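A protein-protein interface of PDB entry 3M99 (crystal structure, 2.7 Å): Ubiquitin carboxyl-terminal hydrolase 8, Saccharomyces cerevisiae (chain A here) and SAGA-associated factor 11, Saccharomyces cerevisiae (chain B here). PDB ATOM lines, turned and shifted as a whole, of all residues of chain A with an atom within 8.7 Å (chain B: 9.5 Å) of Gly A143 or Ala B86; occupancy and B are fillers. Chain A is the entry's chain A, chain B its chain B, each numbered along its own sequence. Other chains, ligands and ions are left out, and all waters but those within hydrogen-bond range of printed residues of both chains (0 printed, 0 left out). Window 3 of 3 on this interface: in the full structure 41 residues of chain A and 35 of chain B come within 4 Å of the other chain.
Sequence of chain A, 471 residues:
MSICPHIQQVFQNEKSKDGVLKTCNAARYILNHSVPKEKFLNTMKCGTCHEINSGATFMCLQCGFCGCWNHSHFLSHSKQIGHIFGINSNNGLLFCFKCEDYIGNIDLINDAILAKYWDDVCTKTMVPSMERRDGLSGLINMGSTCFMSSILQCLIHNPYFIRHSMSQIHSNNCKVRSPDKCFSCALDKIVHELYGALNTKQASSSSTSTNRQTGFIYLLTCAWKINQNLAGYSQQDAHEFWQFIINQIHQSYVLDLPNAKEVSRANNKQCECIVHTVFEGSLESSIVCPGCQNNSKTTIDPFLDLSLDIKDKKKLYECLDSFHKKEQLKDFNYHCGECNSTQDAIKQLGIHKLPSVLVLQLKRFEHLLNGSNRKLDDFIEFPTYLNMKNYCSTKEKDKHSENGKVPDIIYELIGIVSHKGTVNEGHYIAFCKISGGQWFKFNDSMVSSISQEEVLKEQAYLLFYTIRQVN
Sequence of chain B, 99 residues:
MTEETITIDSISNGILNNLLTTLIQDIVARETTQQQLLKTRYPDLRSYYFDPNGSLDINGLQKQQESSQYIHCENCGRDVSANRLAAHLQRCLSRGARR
Of the 17 printed residues of chain B, 8 touch a printed residue of chain A. Hydrophobic or aromatic side chains of chain B within 4 Å of the printed part of chain A: Ile B71, Leu B85, Ala B86, Leu B89 and Leu B93. Among the printed residues, 17 pairs touch across the chains. Among the printed residues, no Asp or Glu carboxylate lies within 4 Å of a Lys or Arg side-chain nitrogen of the other chain.
O of Met A142 sits at hydrogen-bond distance from N of Ala B86 (2.8 Å). The backbone carbonyl oxygen (O) of Asn A141 sits close to the side-chain carboxylate (OE2) of Glu B66 (3.1 Å). The backbone NH (N) of Leu B85 lies within hydrogen-bond range of the backbone carbonyl oxygen (O) of Met A142, 3.4 Å away.
Gly A143 touches just these residues of chain B: Asn B83 (3.9 Å) and Ala B86 (3.97 Å). No residue of chain B comes within 4 Å of Ser A144. Printed residues of chain A within 4 Å of Asn B83: Asn A141 (3.7 Å), Met A142 (3.99 Å) and Gly A143 (3.9 Å). Of the printed residues of chain A, Leu B85 touches Met A142 (3.4 Å) and Ile A217 (3.9 Å). Of the printed residues of chain A, Leu B93 touches Thr A221 (3.9 Å) and Trp A224 (3.8 Å). The nearest residue of chain A that does not touch Ala B86 is Leu A220 (4.9 Å).
Asn A141 touches Asn B83. CD1 of Ile B71 touches CE of Met A142 (3.4 Å). O of Ala B82 touches CA of Met A142 (3.2 Å). Met A142 touches Asn B83 (C to O, 3.99 Å). Gly A143 touches Asn B83 (N to O, 3.9 Å). Ala B86 touches Gly A143. Ala B86 touches Thr A145. OG1 of Thr A221 touches CD1 of Leu B89 (3.95 Å). CG2 of Thr A221 touches CD2 of Leu B93 (3.9 Å). Trp A224 touches Leu B93 (CH2 to C, 3.8 Å).
The backbone NH (N) of Gly A143 is in hydrogen-bond range of the side-chain amide oxygen (OD1) of Asn A141 (2.8 Å). The backbone carbonyl oxygen (O) of Ile A217 lies within hydrogen-bond range of the side-chain hydroxyl (OG1) of Thr A221, 3.3 Å away. OD1 of Asp A444 is in hydrogen-bond range of ND2 of Asn A141 (3.4 Å). The backbone carbonyl oxygen (O) of Val B80 sits at hydrogen-bond distance from the backbone NH (N) of Ile B71 (2.9 Å). The side-chain hydroxyl (OG1) of Thr A145 is in hydrogen-bond range of the backbone NH (N) of Met A142, at 3.0 Å. OD1 of Asn A141 lies within hydrogen-bond range of N of Ser A144, at 3.3 Å.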
ATOM      1  N   ILE A 140       3.190  13.047  10.376  1.00  0.00           N
ATOM      2  CA  ILE A 140       2.793  14.325   9.786  1.00  0.00           C
ATOM      3  C   ILE A 140       1.446  14.782  10.333  1.00  0.00           C
ATOM      4  O   ILE A 140       0.575  13.959  10.611  1.00  0.00           O
ATOM      5  CB  ILE A 140       2.690  14.230   8.246  1.00  0.00           C
ATOM      6  CG1 ILE A 140       4.049  13.888   7.625  1.00  0.00           C
ATOM      7  CG2 ILE A 140       2.146  15.518   7.666  1.00  0.00           C
ATOM      8  CD1 ILE A 140       5.128  14.917   7.888  1.00  0.00           C
ATOM      9  N   ASN A 141       1.274  16.089  10.504  1.00  0.00           N
ATOM     10  CA  ASN A 141      -0.029  16.625  10.896  1.00  0.00           C
ATOM     11  C   ASN A 141      -0.904  16.872   9.680  1.00  0.00           C
ATOM     12  O   ASN A 141      -0.486  17.539   8.737  1.00  0.00           O
ATOM     13  CB  ASN A 141       0.110  17.923  11.688  1.00  0.00           C
ATOM     14  CG  ASN A 141      -1.220  18.412  12.232  1.00  0.00           C
ATOM     15  OD1 ASN A 141      -2.224  18.452  11.517  1.00  0.00           O
ATOM     16  ND2 ASN A 141      -1.235  18.779  13.509  1.00  0.00           N
ATOM     17  N   MET A 142      -2.124  16.351   9.709  1.00  0.00           N
ATOM     18  CA  MET A 142      -2.984  16.424   8.536  1.00  0.00           C
ATOM     19  C   MET A 142      -4.314  17.113   8.801  1.00  0.00           C
ATOM     20  O   MET A 142      -5.307  16.823   8.138  1.00  0.00           O
ATOM     21  CB  MET A 142      -3.231  15.025   7.982  1.00  0.00           C
ATOM     22  CG  MET A 142      -1.970  14.233   7.742  1.00  0.00           C
ATOM     23  SD  MET A 142      -2.367  12.551   7.251  1.00  0.00           S
ATOM     24  CE  MET A 142      -0.774  11.992   6.659  1.00  0.00           C
ATOM     25  N   GLY A 143      -4.336  18.027   9.763  1.00  0.00           N
ATOM     26  CA  GLY A 143      -5.532  18.810  10.017  1.00  0.00           C
ATOM     27  C   GLY A 143      -6.059  18.629  11.421  1.00  0.00           C
ATOM     28  O   GLY A 143      -7.130  18.060  11.626  1.00  0.00           O
ATOM     29  N   SER A 144      -5.301  19.130  12.389  1.00  0.00           N
ATOM     30  CA  SER A 144      -5.596  18.899  13.796  1.00  0.00           C
ATOM     31  C   SER A 144      -5.744  17.395  14.062  1.00  0.00           C
ATOM     32  O   SER A 144      -6.734  16.951  14.646  1.00  0.00           O
ATOM     33  CB  SER A 144      -6.852  19.665  14.218  1.00  0.00           C
ATOM     34  OG  SER A 144      -6.920  19.811  15.626  1.00  0.00           O
ATOM     35  N   THR A 145      -4.751  16.622  13.617  1.00  0.00           N
ATOM     36  CA  THR A 145      -4.728  15.172  13.826  1.00  0.00           C
ATOM     37  C   THR A 145      -3.757  14.757  14.928  1.00  0.00           C
ATOM     38  O   THR A 145      -3.358  13.598  14.998  1.00  0.00           O
ATOM     39  CB  THR A 145      -4.311  14.412  12.548  1.00  0.00           C
ATOM     40  OG1 THR A 145      -3.033  14.884  12.110  1.00  0.00           O
ATOM     41  CG2 THR A 145      -5.325  14.611  11.439  1.00  0.00           C
ATOM     42  N   CYS A 146      -3.370  15.697  15.784  1.00  0.00           N
ATOM     43  CA  CYS A 146      -2.393  15.409  16.829  1.00  0.00           C
ATOM     44  C   CYS A 146      -3.037  14.727  18.030  1.00  0.00           C
ATOM     45  O   CYS A 146      -2.346  14.133  18.853  1.00  0.00           O
ATOM     46  CB  CYS A 146      -1.676  16.688  17.266  1.00  0.00           C
ATOM     47  SG  CYS A 146      -2.771  17.955  17.942  1.00  0.00           S
ATOM     48  N   PHE A 147      -4.362  14.819  18.130  1.00  0.00           N
ATOM     49  CA  PHE A 147      -5.095  14.169  19.217  1.00  0.00           C
ATOM     50  C   PHE A 147      -5.153  12.660  19.000  1.00  0.00           C
ATOM     51  O   PHE A 147      -5.541  11.899  19.889  1.00  0.00           O
ATOM     52  CB  PHE A 147      -6.508  14.747  19.354  1.00  0.00           C
ATOM     53  CG  PHE A 147      -7.489  14.224  18.340  1.00  0.00           C
ATOM     54  CD1 PHE A 147      -8.357  13.189  18.661  1.00  0.00           C
ATOM     55  CD2 PHE A 147      -7.559  14.777  17.073  1.00  0.00           C
ATOM     56  CE1 PHE A 147      -9.272  12.709  17.734  1.00  0.00           C
ATOM     57  CE2 PHE A 147      -8.469  14.304  16.142  1.00  0.00           C
ATOM     58  CZ  PHE A 147      -9.328  13.268  16.475  1.00  0.00           C
ATOM     59  N   MET A 148      -4.764  12.248  17.799  1.00  0.00           N
ATOM     60  CA  MET A 148      -4.669  10.843  17.449  1.00  0.00           C
ATOM     61  C   MET A 148      -3.195  10.469  17.377  1.00  0.00           C
ATOM     62  O   MET A 148      -2.738   9.537  18.039  1.00  0.00           O
ATOM     63  CB  MET A 148      -5.319  10.593  16.088  1.00  0.00           C
ATOM     64  CG  MET A 148      -6.699  11.202  15.914  1.00  0.00           C
ATOM     65  SD  MET A 148      -7.221  11.202  14.182  1.00  0.00           S
ATOM     66  CE  MET A 148      -7.430   9.444  13.897  1.00  0.00           C
ATOM     67  N   PHE A 216      -0.910   5.267   8.474  1.00  0.00           N
ATOM     68  CA  PHE A 216      -1.589   6.253   9.304  1.00  0.00           C
ATOM     69  C   PHE A 216      -2.746   6.891   8.539  1.00  0.00           C
ATOM     70  O   PHE A 216      -3.796   7.188   9.105  1.00  0.00           O
ATOM     71  CB  PHE A 216      -0.596   7.314   9.770  1.00  0.00           C
ATOM     72  CG  PHE A 216      -1.211   8.402  10.596  1.00  0.00           C
ATOM     73  CD1 PHE A 216      -2.078   8.098  11.627  1.00  0.00           C
ATOM     74  CD2 PHE A 216      -0.905   9.730  10.352  1.00  0.00           C
ATOM     75  CE1 PHE A 216      -2.638   9.098  12.393  1.00  0.00           C
ATOM     76  CE2 PHE A 216      -1.463  10.736  11.118  1.00  0.00           C
ATOM     77  CZ  PHE A 216      -2.329  10.419  12.138  1.00  0.00           C
ATOM     78  N   ILE A 217      -2.534   7.096   7.244  1.00  0.00           N
ATOM     79  CA  ILE A 217      -3.578   7.553   6.344  1.00  0.00           C
ATOM     80  C   ILE A 217      -4.678   6.501   6.256  1.00  0.00           C
ATOM     81  O   ILE A 217      -5.859   6.812   6.386  1.00  0.00           O
ATOM     82  CB  ILE A 217      -3.009   7.811   4.939  1.00  0.00           C
ATOM     83  CG1 ILE A 217      -2.044   9.000   4.968  1.00  0.00           C
ATOM     84  CG2 ILE A 217      -4.131   8.040   3.937  1.00  0.00           C
ATOM     85  CD1 ILE A 217      -0.986   8.954   3.877  1.00  0.00           C
ATOM     86  N   LEU A 220      -6.993   6.889   9.018  1.00  0.00           N
ATOM     87  CA  LEU A 220      -7.958   7.966   8.858  1.00  0.00           C
ATOM     88  C   LEU A 220      -9.103   7.479   7.979  1.00  0.00           C
ATOM     89  O   LEU A 220     -10.267   7.558   8.357  1.00  0.00           O
ATOM     90  CB  LEU A 220      -7.296   9.196   8.244  1.00  0.00           C
ATOM     91  CG  LEU A 220      -6.345   9.956   9.168  1.00  0.00           C
ATOM     92  CD1 LEU A 220      -5.636  11.064   8.408  1.00  0.00           C
ATOM     93  CD2 LEU A 220      -7.086  10.514  10.374  1.00  0.00           C
ATOM     94  N   THR A 221      -8.758   6.951   6.811  1.00  0.00           N
ATOM     95  CA  THR A 221      -9.750   6.440   5.874  1.00  0.00           C
ATOM     96  C   THR A 221     -10.683   5.416   6.520  1.00  0.00           C
ATOM     97  O   THR A 221     -11.859   5.332   6.170  1.00  0.00           O
ATOM     98  CB  THR A 221      -9.082   5.815   4.634  1.00  0.00           C
ATOM     99  OG1 THR A 221      -8.168   6.756   4.057  1.00  0.00           O
ATOM    100  CG2 THR A 221     -10.125   5.435   3.595  1.00  0.00           C
ATOM    101  N   TRP A 224     -12.997   7.108   9.265  1.00  0.00           N
ATOM    102  CA  TRP A 224     -14.085   7.890   8.673  1.00  0.00           C
ATOM    103  C   TRP A 224     -15.397   7.117   8.520  1.00  0.00           C
ATOM    104  O   TRP A 224     -16.463   7.617   8.886  1.00  0.00           O
ATOM    105  CB  TRP A 224     -13.680   8.473   7.320  1.00  0.00           C
ATOM    106  CG  TRP A 224     -14.819   9.164   6.652  1.00  0.00           C
ATOM    107  CD1 TRP A 224     -15.210  10.458   6.834  1.00  0.00           C
ATOM    108  CD2 TRP A 224     -15.740   8.591   5.714  1.00  0.00           C
ATOM    109  NE1 TRP A 224     -16.311  10.732   6.057  1.00  0.00           N
ATOM    110  CE2 TRP A 224     -16.657   9.604   5.362  1.00  0.00           C
ATOM    111  CE3 TRP A 224     -15.874   7.326   5.134  1.00  0.00           C
ATOM    112  CZ2 TRP A 224     -17.695   9.387   4.454  1.00  0.00           C
ATOM    113  CZ3 TRP A 224     -16.906   7.112   4.234  1.00  0.00           C
ATOM    114  CH2 TRP A 224     -17.803   8.138   3.902  1.00  0.00           C
ATOM    115  N   GLN A 235     -12.548  15.186  17.901  1.00  0.00           N
ATOM    116  CA  GLN A 235     -12.058  16.393  17.243  1.00  0.00           C
ATOM    117  C   GLN A 235     -11.174  17.206  18.177  1.00  0.00           C
ATOM    118  O   GLN A 235     -10.285  17.937  17.732  1.00  0.00           O
ATOM    119  CB  GLN A 235     -13.226  17.261  16.779  1.00  0.00           C
ATOM    120  CG  GLN A 235     -13.990  16.716  15.591  1.00  0.00           C
ATOM    121  CD  GLN A 235     -14.892  17.766  14.982  1.00  0.00           C
ATOM    122  OE1 GLN A 235     -14.814  18.942  15.338  1.00  0.00           O
ATOM    123  NE2 GLN A 235     -15.752  17.352  14.057  1.00  0.00           N
ATOM    124  N   ASP A 444       4.887  16.551  16.160  1.00  0.00           N
ATOM    125  CA  ASP A 444       4.028  15.995  15.136  1.00  0.00           C
ATOM    126  C   ASP A 444       4.892  15.018  14.367  1.00  0.00           C
ATOM    127  O   ASP A 444       4.925  13.826  14.665  1.00  0.00           O
ATOM    128  CB  ASP A 444       3.492  17.096  14.219  1.00  0.00           C
ATOM    129  CG  ASP A 444       2.186  17.688  14.716  1.00  0.00           C
ATOM    130  OD1 ASP A 444       1.227  16.910  14.911  1.00  0.00           O
ATOM    131  OD2 ASP A 444       2.110  18.927  14.896  1.00  0.00           O
ATOM    132  N   GLU B  66       6.051  21.683   6.270  1.00  0.00           N
ATOM    133  CA  GLU B  66       5.531  20.998   5.084  1.00  0.00           C
ATOM    134  C   GLU B  66       4.328  21.825   4.631  1.00  0.00           C
ATOM    135  O   GLU B  66       3.327  21.912   5.351  1.00  0.00           O
ATOM    136  CB  GLU B  66       4.384  20.044   5.453  1.00  0.00           C
ATOM    137  CG  GLU B  66       3.422  20.549   6.527  1.00  0.00           C
ATOM    138  CD  GLU B  66       2.679  19.407   7.207  1.00  0.00           C
ATOM    139  OE1 GLU B  66       3.125  18.248   7.061  1.00  0.00           O
ATOM    140  OE2 GLU B  66       1.658  19.661   7.887  1.00  0.00           O
ATOM    141  N   ILE B  71       0.047  14.516  -0.530  1.00  0.00           N
ATOM    142  CA  ILE B  71      -0.231  13.102  -0.338  1.00  0.00           C
ATOM    143  C   ILE B  71      -1.229  12.620  -1.374  1.00  0.00           C
ATOM    144  O   ILE B  71      -2.313  13.177  -1.498  1.00  0.00           O
ATOM    145  CB  ILE B  71      -0.807  12.829   1.047  1.00  0.00           C
ATOM    146  CG1 ILE B  71       0.004  13.569   2.108  1.00  0.00           C
ATOM    147  CG2 ILE B  71      -0.814  11.341   1.317  1.00  0.00           C
ATOM    148  CD1 ILE B  71      -0.488  13.349   3.507  1.00  0.00           C
ATOM    149  N   CYS B  73      -4.126  11.016  -2.678  1.00  0.00           N
ATOM    150  CA  CYS B  73      -5.360  10.437  -2.152  1.00  0.00           C
ATOM    151  C   CYS B  73      -5.856   9.317  -3.055  1.00  0.00           C
ATOM    152  O   CYS B  73      -5.969   9.483  -4.265  1.00  0.00           O
ATOM    153  CB  CYS B  73      -6.435  11.512  -1.990  1.00  0.00           C
ATOM    154  SG  CYS B  73      -7.951  10.958  -1.174  1.00  0.00           S
ATOM    155  N   VAL B  80      -2.955  16.024  -2.376  1.00  0.00           N
ATOM    156  CA  VAL B  80      -3.616  16.879  -1.407  1.00  0.00           C
ATOM    157  C   VAL B  80      -2.582  17.410  -0.445  1.00  0.00           C
ATOM    158  O   VAL B  80      -1.783  16.651   0.092  1.00  0.00           O
ATOM    159  CB  VAL B  80      -4.687  16.095  -0.616  1.00  0.00           C
ATOM    160  CG1 VAL B  80      -5.258  16.934   0.503  1.00  0.00           C
ATOM    161  CG2 VAL B  80      -5.785  15.624  -1.541  1.00  0.00           C
ATOM    162  N   SER B  81      -2.579  18.715  -0.227  1.00  0.00           N
ATOM    163  CA  SER B  81      -1.632  19.272   0.718  1.00  0.00           C
ATOM    164  C   SER B  81      -1.739  18.506   2.031  1.00  0.00           C
ATOM    165  O   SER B  81      -2.812  18.406   2.613  1.00  0.00           O
ATOM    166  CB  SER B  81      -1.873  20.766   0.918  1.00  0.00           C
ATOM    167  OG  SER B  81      -1.285  21.510  -0.136  1.00  0.00           O
ATOM    168  N   ALA B  82      -0.622  17.946   2.477  1.00  0.00           N
ATOM    169  CA  ALA B  82      -0.602  17.149   3.692  1.00  0.00           C
ATOM    170  C   ALA B  82      -1.381  17.812   4.826  1.00  0.00           C
ATOM    171  O   ALA B  82      -2.125  17.148   5.539  1.00  0.00           O
ATOM    172  CB  ALA B  82       0.826  16.867   4.118  1.00  0.00           C
ATOM    173  N   ASN B  83      -1.227  19.121   4.987  1.00  0.00           N
ATOM    174  CA  ASN B  83      -1.868  19.812   6.105  1.00  0.00           C
ATOM    175  C   ASN B  83      -3.389  19.907   5.967  1.00  0.00           C
ATOM    176  O   ASN B  83      -4.057  20.549   6.780  1.00  0.00           O
ATOM    177  CB  ASN B  83      -1.260  21.206   6.310  1.00  0.00           C
ATOM    178  CG  ASN B  83      -1.436  22.110   5.097  1.00  0.00           C
ATOM    179  OD1 ASN B  83      -0.917  21.825   4.016  1.00  0.00           O
ATOM    180  ND2 ASN B  83      -2.165  23.212   5.278  1.00  0.00           N
ATOM    181  N   ARG B  84      -3.928  19.261   4.940  1.00  0.00           N
ATOM    182  CA  ARG B  84      -5.358  19.308   4.664  1.00  0.00           C
ATOM    183  C   ARG B  84      -5.905  17.980   4.176  1.00  0.00           C
ATOM    184  O   ARG B  84      -6.782  17.954   3.325  1.00  0.00           O
ATOM    185  CB  ARG B  84      -5.654  20.356   3.596  1.00  0.00           C
ATOM    186  CG  ARG B  84      -6.155  21.682   4.131  1.00  0.00           C
ATOM    187  CD  ARG B  84      -6.636  22.577   2.999  1.00  0.00           C
ATOM    188  NE  ARG B  84      -7.649  23.518   3.468  1.00  0.00           N
ATOM    189  CZ  ARG B  84      -8.953  23.275   3.442  1.00  0.00           C
ATOM    190  NH1 ARG B  84      -9.407  22.125   2.962  1.00  0.00           N
ATOM    191  NH2 ARG B  84      -9.800  24.184   3.898  1.00  0.00           N
ATOM    192  N   LEU B  85      -5.390  16.876   4.699  1.00  0.00           N
ATOM    193  CA  LEU B  85      -5.848  15.567   4.256  1.00  0.00           C
ATOM    194  C   LEU B  85      -7.038  15.112   5.078  1.00  0.00           C
ATOM    195  O   LEU B  85      -7.929  14.442   4.567  1.00  0.00           O
ATOM    196  CB  LEU B  85      -4.730  14.532   4.342  1.00  0.00           C
ATOM    197  CG  LEU B  85      -5.120  13.148   3.821  1.00  0.00           C
ATOM    198  CD1 LEU B  85      -5.554  13.223   2.369  1.00  0.00           C
ATOM    199  CD2 LEU B  85      -3.968  12.188   3.984  1.00  0.00           C
ATOM    200  N   ALA B  86      -7.048  15.475   6.357  1.00  0.00           N
ATOM    201  CA  ALA B  86      -8.159  15.126   7.236  1.00  0.00           C
ATOM    202  C   ALA B  86      -9.429  15.809   6.765  1.00  0.00           C
ATOM    203  O   ALA B  86     -10.484  15.182   6.673  1.00  0.00           O
ATOM    204  CB  ALA B  86      -7.853  15.517   8.669  1.00  0.00           C
ATOM    205  N   ALA B  87      -9.319  17.099   6.464  1.00  0.00           N
ATOM    206  CA  ALA B  87     -10.453  17.867   5.980  1.00  0.00           C
ATOM    207  C   ALA B  87     -10.879  17.377   4.602  1.00  0.00           C
ATOM    208  O   ALA B  87     -12.067  17.339   4.283  1.00  0.00           O
ATOM    209  CB  ALA B  87     -10.103  19.336   5.936  1.00  0.00           C
ATOM    210  N   HIS B  88      -9.903  16.996   3.789  1.00  0.00           N
ATOM    211  CA  HIS B  88     -10.173  16.556   2.426  1.00  0.00           C
ATOM    212  C   HIS B  88     -10.946  15.239   2.379  1.00  0.00           C
ATOM    213  O   HIS B  88     -11.799  15.048   1.515  1.00  0.00           O
ATOM    214  CB  HIS B  88      -8.868  16.447   1.637  1.00  0.00           C
ATOM    215  CG  HIS B  88      -9.008  15.756   0.325  1.00  0.00           C
ATOM    216  ND1 HIS B  88      -9.257  16.432  -0.858  1.00  0.00           N
ATOM    217  CD2 HIS B  88      -8.921  14.447  -0.013  1.00  0.00           C
ATOM    218  CE1 HIS B  88      -9.323  15.570  -1.848  1.00  0.00           C
ATOM    219  NE2 HIS B  88      -9.123  14.357  -1.368  1.00  0.00           N
ATOM    220  N   LEU B  89     -10.652  14.334   3.308  1.00  0.00           N
ATOM    221  CA  LEU B  89     -11.307  13.029   3.333  1.00  0.00           C
ATOM    222  C   LEU B  89     -12.747  13.149   3.811  1.00  0.00           C
ATOM    223  O   LEU B  89     -13.627  12.406   3.374  1.00  0.00           O
ATOM    224  CB  LEU B  89     -10.537  12.057   4.229  1.00  0.00           C
ATOM    225  CG  LEU B  89      -9.201  11.554   3.684  1.00  0.00           C
ATOM    226  CD1 LEU B  89      -8.528  10.640   4.689  1.00  0.00           C
ATOM    227  CD2 LEU B  89      -9.398  10.839   2.361  1.00  0.00           C
ATOM    228  N   GLN B  90     -12.983  14.101   4.703  1.00  0.00           N
ATOM    229  CA  GLN B  90     -14.312  14.328   5.244  1.00  0.00           C
ATOM    230  C   GLN B  90     -15.306  14.853   4.210  1.00  0.00           C
ATOM    231  O   GLN B  90     -16.464  15.098   4.538  1.00  0.00           O
ATOM    232  CB  GLN B  90     -14.246  15.261   6.454  1.00  0.00           C
ATOM    233  CG  GLN B  90     -13.616  14.597   7.669  1.00  0.00           C
ATOM    234  CD  GLN B  90     -13.518  15.515   8.872  1.00  0.00           C
ATOM    235  OE1 GLN B  90     -13.478  16.741   8.738  1.00  0.00           O
ATOM    236  NE2 GLN B  90     -13.466  14.921  10.064  1.00  0.00           N
ATOM    237  N   ARG B  91     -14.857  15.020   2.969  1.00  0.00           N
ATOM    238  CA  ARG B  91     -15.754  15.416   1.883  1.00  0.00           C
ATOM    239  C   ARG B  91     -15.384  14.793   0.535  1.00  0.00           C
ATOM    240  O   ARG B  91     -16.005  15.089  -0.486  1.00  0.00           O
ATOM    241  CB  ARG B  91     -15.864  16.941   1.776  1.00  0.00           C
ATOM    242  CG  ARG B  91     -14.626  17.699   2.196  1.00  0.00           C
ATOM    243  CD  ARG B  91     -14.761  19.199   1.927  1.00  0.00           C
ATOM    244  NE  ARG B  91     -13.481  19.880   2.120  1.00  0.00           N
ATOM    245  CZ  ARG B  91     -12.523  19.948   1.199  1.00  0.00           C
ATOM    246  NH1 ARG B  91     -12.698  19.391   0.007  1.00  0.00           N
ATOM    247  NH2 ARG B  91     -11.387  20.578   1.469  1.00  0.00           N
ATOM    248  N   CYS B  92     -14.377  13.926   0.549  1.00  0.00           N
ATOM    249  CA  CYS B  92     -13.953  13.187  -0.634  1.00  0.00           C
ATOM    250  C   CYS B  92     -14.527  11.783  -0.549  1.00  0.00           C
ATOM    251  O   CYS B  92     -15.020  11.239  -1.534  1.00  0.00           O
ATOM    252  CB  CYS B  92     -12.418  13.126  -0.703  1.00  0.00           C
ATOM    253  SG  CYS B  92     -11.664  12.300  -2.165  1.00  0.00           S
ATOM    254  N   LEU B  93     -14.464  11.203   0.644  1.00  0.00           N
ATOM    255  CA  LEU B  93     -14.950   9.849   0.860  1.00  0.00           C
ATOM    256  C   LEU B  93     -16.472   9.800   0.794  1.00  0.00           C
ATOM    257  O   LEU B  93     -17.049   8.903   0.174  1.00  0.00           O
ATOM    258  CB  LEU B  93     -14.447   9.311   2.202  1.00  0.00           C
ATOM    259  CG  LEU B  93     -12.977   8.875   2.256  1.00  0.00           C
ATOM    260  CD1 LEU B  93     -12.433   8.929   3.678  1.00  0.00           C
ATOM    261  CD2 LEU B  93     -12.799   7.484   1.667  1.00  0.00           C
